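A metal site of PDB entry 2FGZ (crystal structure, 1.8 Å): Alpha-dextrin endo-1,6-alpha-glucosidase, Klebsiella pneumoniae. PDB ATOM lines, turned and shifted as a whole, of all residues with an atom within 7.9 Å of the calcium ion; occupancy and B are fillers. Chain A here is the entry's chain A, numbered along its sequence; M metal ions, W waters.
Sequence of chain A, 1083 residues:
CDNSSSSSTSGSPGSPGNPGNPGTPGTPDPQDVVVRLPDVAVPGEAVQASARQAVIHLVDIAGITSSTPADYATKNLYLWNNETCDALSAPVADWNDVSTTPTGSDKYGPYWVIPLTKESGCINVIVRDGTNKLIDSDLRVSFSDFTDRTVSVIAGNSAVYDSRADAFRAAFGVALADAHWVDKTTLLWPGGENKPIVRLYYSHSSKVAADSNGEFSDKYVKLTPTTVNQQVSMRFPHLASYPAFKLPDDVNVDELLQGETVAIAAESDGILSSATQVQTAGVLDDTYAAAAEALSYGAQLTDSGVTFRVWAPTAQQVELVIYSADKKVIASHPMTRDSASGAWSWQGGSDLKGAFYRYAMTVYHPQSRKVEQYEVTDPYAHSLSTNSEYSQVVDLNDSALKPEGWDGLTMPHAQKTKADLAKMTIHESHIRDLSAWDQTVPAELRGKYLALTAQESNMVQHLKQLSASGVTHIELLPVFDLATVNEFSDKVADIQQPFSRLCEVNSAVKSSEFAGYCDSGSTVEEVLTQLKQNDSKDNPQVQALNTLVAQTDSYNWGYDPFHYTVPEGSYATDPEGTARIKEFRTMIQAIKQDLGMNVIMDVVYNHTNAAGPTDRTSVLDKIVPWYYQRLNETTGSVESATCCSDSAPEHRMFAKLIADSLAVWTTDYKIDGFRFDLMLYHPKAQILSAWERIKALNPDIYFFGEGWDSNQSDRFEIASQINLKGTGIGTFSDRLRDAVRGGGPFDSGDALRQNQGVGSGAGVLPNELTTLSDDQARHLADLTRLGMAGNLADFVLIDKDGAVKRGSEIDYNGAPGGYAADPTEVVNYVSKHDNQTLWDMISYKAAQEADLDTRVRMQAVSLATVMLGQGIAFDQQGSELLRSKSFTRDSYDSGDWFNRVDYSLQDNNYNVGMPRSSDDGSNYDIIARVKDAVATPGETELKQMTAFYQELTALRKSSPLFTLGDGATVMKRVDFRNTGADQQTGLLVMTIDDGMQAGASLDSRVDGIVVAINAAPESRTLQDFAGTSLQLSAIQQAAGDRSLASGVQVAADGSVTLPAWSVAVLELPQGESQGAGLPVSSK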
ATOM      1  N   THR A 484     -19.569 -12.338   1.874  1.00  0.00           N
ATOM      2  CA  THR A 484     -19.171 -11.504   3.003  1.00  0.00           C
ATOM      3  C   THR A 484     -19.587 -11.837   4.437  1.00  0.00           C
ATOM      4  O   THR A 484     -19.538 -10.978   5.319  1.00  0.00           O
ATOM      5  CB  THR A 484     -19.564 -10.058   2.706  1.00  0.00           C
ATOM      6  OG1 THR A 484     -20.908 -10.021   2.219  1.00  0.00           O
ATOM      7  CG2 THR A 484     -18.634  -9.482   1.639  1.00  0.00           C
ATOM      8  N   VAL A 485     -19.982 -13.080   4.657  1.00  0.00           N
ATOM      9  CA  VAL A 485     -20.326 -13.551   5.998  1.00  0.00           C
ATOM     10  C   VAL A 485     -19.702 -14.945   6.081  1.00  0.00           C
ATOM     11  O   VAL A 485     -19.894 -15.763   5.171  1.00  0.00           O
ATOM     12  CB  VAL A 485     -21.846 -13.674   6.231  1.00  0.00           C
ATOM     13  CG1 VAL A 485     -22.113 -14.415   7.532  1.00  0.00           C
ATOM     14  CG2 VAL A 485     -22.482 -12.295   6.291  1.00  0.00           C
ATOM     15  N   ASN A 486     -18.953 -15.204   7.139  1.00  0.00           N
ATOM     16  CA  ASN A 486     -18.328 -16.518   7.296  1.00  0.00           C
ATOM     17  C   ASN A 486     -19.394 -17.478   7.793  1.00  0.00           C
ATOM     18  O   ASN A 486     -20.035 -17.235   8.820  1.00  0.00           O
ATOM     19  CB  ASN A 486     -17.172 -16.446   8.307  1.00  0.00           C
ATOM     20  CG  ASN A 486     -16.276 -17.679   8.237  1.00  0.00           C
ATOM     21  OD1 ASN A 486     -16.762 -18.806   8.151  1.00  0.00           O
ATOM     22  ND2 ASN A 486     -14.965 -17.462   8.296  1.00  0.00           N
ATOM     23  N   ASP A 494     -21.293 -12.298  17.286  1.00  0.00           N
ATOM     24  CA  ASP A 494     -22.346 -11.308  17.126  1.00  0.00           C
ATOM     25  C   ASP A 494     -22.478 -10.503  18.416  1.00  0.00           C
ATOM     26  O   ASP A 494     -21.975 -10.912  19.458  1.00  0.00           O
ATOM     27  CB  ASP A 494     -23.661 -11.997  16.745  1.00  0.00           C
ATOM     28  CG  ASP A 494     -23.673 -12.417  15.270  1.00  0.00           C
ATOM     29  OD1 ASP A 494     -23.624 -11.518  14.410  1.00  0.00           O
ATOM     30  OD2 ASP A 494     -23.725 -13.626  14.984  1.00  0.00           O
ATOM     31  N   ASN A 546     -18.189  -0.708  16.660  1.00  0.00           N
ATOM     32  CA  ASN A 546     -19.012  -1.442  15.699  1.00  0.00           C
ATOM     33  C   ASN A 546     -18.307  -1.713  14.379  1.00  0.00           C
ATOM     34  O   ASN A 546     -18.545  -2.740  13.756  1.00  0.00           O
ATOM     35  CB  ASN A 546     -20.319  -0.700  15.435  1.00  0.00           C
ATOM     36  CG  ASN A 546     -21.389  -1.614  14.870  1.00  0.00           C
ATOM     37  OD1 ASN A 546     -21.740  -2.616  15.496  1.00  0.00           O
ATOM     38  ND2 ASN A 546     -21.912  -1.290  13.696  1.00  0.00           N
ATOM     39  N   THR A 547     -17.454  -0.799  13.953  1.00  0.00           N
ATOM     40  CA  THR A 547     -16.726  -0.975  12.695  1.00  0.00           C
ATOM     41  C   THR A 547     -15.856  -2.220  12.772  1.00  0.00           C
ATOM     42  O   THR A 547     -15.675  -2.936  11.780  1.00  0.00           O
ATOM     43  CB  THR A 547     -15.857   0.259  12.382  1.00  0.00           C
ATOM     44  OG1 THR A 547     -16.713   1.382  12.138  1.00  0.00           O
ATOM     45  CG2 THR A 547     -14.983   0.007  11.160  1.00  0.00           C
ATOM     46  N   LEU A 548     -15.312  -2.491  13.954  1.00  0.00           N
ATOM     47  CA  LEU A 548     -14.479  -3.658  14.153  1.00  0.00           C
ATOM     48  C   LEU A 548     -15.365  -4.903  14.242  1.00  0.00           C
ATOM     49  O   LEU A 548     -15.055  -5.951  13.680  1.00  0.00           O
ATOM     50  CB  LEU A 548     -13.667  -3.506  15.443  1.00  0.00           C
ATOM     51  CG  LEU A 548     -12.749  -2.282  15.472  1.00  0.00           C
ATOM     52  CD1 LEU A 548     -12.045  -2.196  16.824  1.00  0.00           C
ATOM     53  CD2 LEU A 548     -11.726  -2.390  14.350  1.00  0.00           C
ATOM     54  N   VAL A 549     -16.490  -4.767  14.936  1.00  0.00           N
ATOM     55  CA  VAL A 549     -17.433  -5.863  15.086  1.00  0.00           C
ATOM     56  C   VAL A 549     -17.908  -6.341  13.712  1.00  0.00           C
ATOM     57  O   VAL A 549     -18.061  -7.535  13.480  1.00  0.00           O
ATOM     58  CB  VAL A 549     -18.672  -5.430  15.925  1.00  0.00           C
ATOM     59  CG1 VAL A 549     -19.748  -6.512  15.874  1.00  0.00           C
ATOM     60  CG2 VAL A 549     -18.253  -5.154  17.375  1.00  0.00           C
ATOM     61  N   ALA A 550     -18.130  -5.386  12.811  1.00  0.00           N
ATOM     62  CA  ALA A 550     -18.622  -5.686  11.462  1.00  0.00           C
ATOM     63  C   ALA A 550     -17.773  -6.664  10.667  1.00  0.00           C
ATOM     64  O   ALA A 550     -18.271  -7.337   9.768  1.00  0.00           O
ATOM     65  CB  ALA A 550     -18.766  -4.378  10.684  1.00  0.00           C
ATOM     66  N   GLN A 551     -16.480  -6.737  10.984  1.00  0.00           N
ATOM     67  CA  GLN A 551     -15.553  -7.626  10.288  1.00  0.00           C
ATOM     68  C   GLN A 551     -15.797  -9.105  10.518  1.00  0.00           C
ATOM     69  O   GLN A 551     -15.489  -9.931   9.650  1.00  0.00           O
ATOM     70  CB  GLN A 551     -14.117  -7.296  10.687  1.00  0.00           C
ATOM     71  CG  GLN A 551     -13.716  -5.847  10.475  1.00  0.00           C
ATOM     72  CD  GLN A 551     -12.383  -5.508  11.122  1.00  0.00           C
ATOM     73  OE1 GLN A 551     -11.877  -4.391  10.981  1.00  0.00           O
ATOM     74  NE2 GLN A 551     -11.817  -6.463  11.840  1.00  0.00           N
ATOM     75  N   THR A 552     -16.343  -9.449  11.680  1.00  0.00           N
ATOM     76  CA  THR A 552     -16.568 -10.858  12.025  1.00  0.00           C
ATOM     77  C   THR A 552     -17.964 -11.213  12.523  1.00  0.00           C
ATOM     78  O   THR A 552     -18.135 -12.253  13.173  1.00  0.00           O
ATOM     79  CB  THR A 552     -15.522 -11.308  13.070  1.00  0.00           C
ATOM     80  OG1 THR A 552     -15.492 -10.353  14.150  1.00  0.00           O
ATOM     81  CG2 THR A 552     -14.131 -11.389  12.450  1.00  0.00           C
ATOM     82  N   ASP A 553     -18.973 -10.398  12.226  1.00  0.00           N
ATOM     83  CA  ASP A 553     -20.326 -10.712  12.661  1.00  0.00           C
ATOM     84  C   ASP A 553     -21.090 -11.470  11.563  1.00  0.00           C
ATOM     85  O   ASP A 553     -20.524 -11.820  10.533  1.00  0.00           O
ATOM     86  CB  ASP A 553     -21.098  -9.454  13.101  1.00  0.00           C
ATOM     87  CG  ASP A 553     -21.279  -8.442  11.976  1.00  0.00           C
ATOM     88  OD1 ASP A 553     -21.083  -8.791  10.792  1.00  0.00           O
ATOM     89  OD2 ASP A 553     -21.640  -7.281  12.274  1.00  0.00           O
ATOM     90  N   SER A 554     -22.371 -11.714  11.792  1.00  0.00           N
ATOM     91  CA  SER A 554     -23.189 -12.432  10.813  1.00  0.00           C
ATOM     92  C   SER A 554     -23.912 -11.482   9.876  1.00  0.00           C
ATOM     93  O   SER A 554     -24.746 -11.915   9.076  1.00  0.00           O
ATOM     94  CB  SER A 554     -24.234 -13.289  11.536  1.00  0.00           C
ATOM     95  OG  SER A 554     -23.653 -14.264  12.389  1.00  0.00           O
ATOM     96  N   TYR A 555     -23.577 -10.194   9.953  1.00  0.00           N
ATOM     97  CA  TYR A 555     -24.280  -9.184   9.167  1.00  0.00           C
ATOM     98  C   TYR A 555     -23.684  -8.581   7.901  1.00  0.00           C
ATOM     99  O   TYR A 555     -22.540  -8.142   7.881  1.00  0.00           O
ATOM    100  CB  TYR A 555     -24.669  -8.015  10.086  1.00  0.00           C
ATOM    101  CG  TYR A 555     -25.749  -7.154   9.498  1.00  0.00           C
ATOM    102  CD1 TYR A 555     -25.482  -6.288   8.435  1.00  0.00           C
ATOM    103  CD2 TYR A 555     -27.067  -7.265   9.942  1.00  0.00           C
ATOM    104  CE1 TYR A 555     -26.510  -5.578   7.822  1.00  0.00           C
ATOM    105  CE2 TYR A 555     -28.102  -6.559   9.334  1.00  0.00           C
ATOM    106  CZ  TYR A 555     -27.809  -5.712   8.267  1.00  0.00           C
ATOM    107  OH  TYR A 555     -28.837  -5.053   7.638  1.00  0.00           O
ATOM    108  N   ASN A 556     -24.506  -8.552   6.856  1.00  0.00           N
ATOM    109  CA  ASN A 556     -24.165  -7.929   5.577  1.00  0.00           C
ATOM    110  C   ASN A 556     -25.375  -8.012   4.668  1.00  0.00           C
ATOM    111  O   ASN A 556     -26.104  -9.004   4.683  1.00  0.00           O
ATOM    112  CB  ASN A 556     -22.965  -8.623   4.906  1.00  0.00           C
ATOM    113  CG  ASN A 556     -22.292  -7.724   3.871  1.00  0.00           C
ATOM    114  OD1 ASN A 556     -22.861  -7.429   2.813  1.00  0.00           O
ATOM    115  ND2 ASN A 556     -21.075  -7.289   4.172  1.00  0.00           N
ATOM    116  N   TRP A 557     -25.633  -6.952   3.902  1.00  0.00           N
ATOM    117  CA  TRP A 557     -26.755  -6.958   2.957  1.00  0.00           C
ATOM    118  C   TRP A 557     -26.594  -8.137   2.013  1.00  0.00           C
ATOM    119  O   TRP A 557     -27.579  -8.766   1.613  1.00  0.00           O
ATOM    120  CB  TRP A 557     -26.797  -5.673   2.137  1.00  0.00           C
ATOM    121  CG  TRP A 557     -27.332  -4.486   2.859  1.00  0.00           C
ATOM    122  CD1 TRP A 557     -28.010  -4.477   4.043  1.00  0.00           C
ATOM    123  CD2 TRP A 557     -27.249  -3.126   2.426  1.00  0.00           C
ATOM    124  NE1 TRP A 557     -28.355  -3.190   4.383  1.00  0.00           N
ATOM    125  CE2 TRP A 557     -27.898  -2.339   3.410  1.00  0.00           C
ATOM    126  CE3 TRP A 557     -26.692  -2.495   1.310  1.00  0.00           C
ATOM    127  CZ2 TRP A 557     -28.004  -0.955   3.307  1.00  0.00           C
ATOM    128  CZ3 TRP A 557     -26.797  -1.111   1.206  1.00  0.00           C
ATOM    129  CH2 TRP A 557     -27.449  -0.350   2.201  1.00  0.00           C
ATOM    130  N   TYR A 892     -24.874  -1.212   4.747  1.00  0.00           N
ATOM    131  CA  TYR A 892     -24.604  -2.585   4.317  1.00  0.00           C
ATOM    132  C   TYR A 892     -23.773  -3.454   5.256  1.00  0.00           C
ATOM    133  O   TYR A 892     -23.947  -4.676   5.298  1.00  0.00           O
ATOM    134  CB  TYR A 892     -23.939  -2.589   2.936  1.00  0.00           C
ATOM    135  CG  TYR A 892     -22.456  -2.331   2.940  1.00  0.00           C
ATOM    136  CD1 TYR A 892     -21.955  -1.048   3.170  1.00  0.00           C
ATOM    137  CD2 TYR A 892     -21.549  -3.362   2.721  1.00  0.00           C
ATOM    138  CE1 TYR A 892     -20.577  -0.807   3.185  1.00  0.00           C
ATOM    139  CE2 TYR A 892     -20.180  -3.140   2.723  1.00  0.00           C
ATOM    140  CZ  TYR A 892     -19.699  -1.860   2.962  1.00  0.00           C
ATOM    141  OH  TYR A 892     -18.336  -1.643   2.968  1.00  0.00           O
ATOM    142  N   ASP A 893     -22.860  -2.838   5.999  1.00  0.00           N
ATOM    143  CA  ASP A 893     -21.991  -3.579   6.904  1.00  0.00           C
ATOM    144  C   ASP A 893     -22.011  -2.923   8.291  1.00  0.00           C
ATOM    145  O   ASP A 893     -21.061  -3.058   9.056  1.00  0.00           O
ATOM    146  CB  ASP A 893     -20.561  -3.578   6.354  1.00  0.00           C
ATOM    147  CG  ASP A 893     -19.718  -4.733   6.880  1.00  0.00           C
ATOM    148  OD1 ASP A 893     -18.492  -4.733   6.629  1.00  0.00           O
ATOM    149  OD2 ASP A 893     -20.270  -5.647   7.529  1.00  0.00           O
ATOM    150  N   SER A 894     -23.105  -2.231   8.589  1.00  0.00           N
ATOM    151  CA  SER A 894     -23.247  -1.547   9.878  1.00  0.00           C
ATOM    152  C   SER A 894     -23.834  -2.427  10.986  1.00  0.00           C
ATOM    153  O   SER A 894     -24.175  -1.930  12.064  1.00  0.00           O
ATOM    154  CB  SER A 894     -24.065  -0.266   9.725  1.00  0.00           C
ATOM    155  OG  SER A 894     -23.316   0.693   9.000  1.00  0.00           O
ATOM    156  N   GLY A 895     -23.946  -3.719  10.705  1.00  0.00           N
ATOM    157  CA  GLY A 895     -24.426  -4.688  11.680  1.00  0.00           C
ATOM    158  C   GLY A 895     -25.831  -4.595  12.246  1.00  0.00           C
ATOM    159  O   GLY A 895     -26.656  -3.799  11.797  1.00  0.00           O
ATOM    160  N   ASP A 896     -26.084  -5.441  13.242  1.00  0.00           N
ATOM    161  CA  ASP A 896     -27.390  -5.481  13.904  1.00  0.00           C
ATOM    162  C   ASP A 896     -27.676  -4.157  14.611  1.00  0.00           C
ATOM    163  O   ASP A 896     -28.823  -3.740  14.719  1.00  0.00           O
ATOM    164  CB  ASP A 896     -27.452  -6.580  14.979  1.00  0.00           C
ATOM    165  CG  ASP A 896     -27.406  -7.981  14.397  1.00  0.00           C
ATOM    166  OD1 ASP A 896     -27.829  -8.195  13.240  1.00  0.00           O
ATOM    167  OD2 ASP A 896     -26.971  -8.896  15.128  1.00  0.00           O
HETATM  168 CA    CA M   1     -20.426  -7.719   8.669  1.00  0.00          CA
HETATM  169  O   HOH W   1     -19.829 -10.022   8.548  1.00  0.00           O
HETATM  170  O   HOH W   2     -21.627  -5.904   9.954  1.00  0.00           O
HETATM  171  O   HOH W   3     -19.534  -8.323   6.375  1.00  0.00           O
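O of Tyr 555 is bound to the calcium ion (2.3 Å). The side-chain carboxylate (OD2) of Asp 893 is bound to the calcium ion, at 2.4 Å. The calcium ion is bound by water W1, 2.4 Å away. The calcium ion is bound by O of Ala 550, 2.4 Å away. The calcium ion is bound by OD1 of Asp 553, 2.5 Å away. The calcium ion is bound by water W2 (2.5 Å). Water W3 binds the calcium ion, 2.5 Å away. The calcium ion has seven donor atoms within binding distance.
Water W1 lies within hydrogen-bond range of the backbone carbonyl oxygen of Asp 553 (2.8 Å) and the backbone carbonyl oxygen of Thr 484 (3.4 Å). Water W3 bridges O of Thr 484 (2.9 Å) and ND2 of Asn 556 (2.9 Å). Water W2 lies within hydrogen-bond range of OD2 of Asp 553 (2.7 Å), O of Asp 893 (3.0 Å) and N of Gly 895 (3.3 Å).
Within 4 Å of the calcium ion: Ala 550, Asp 553, Tyr 555 and Asp 893. Along chain A the residues within 4 Å of the calcium ion span positions 550 to 893. The nearest printed residue that does not touch the calcium ion is Asn 556 (4.5 Å).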
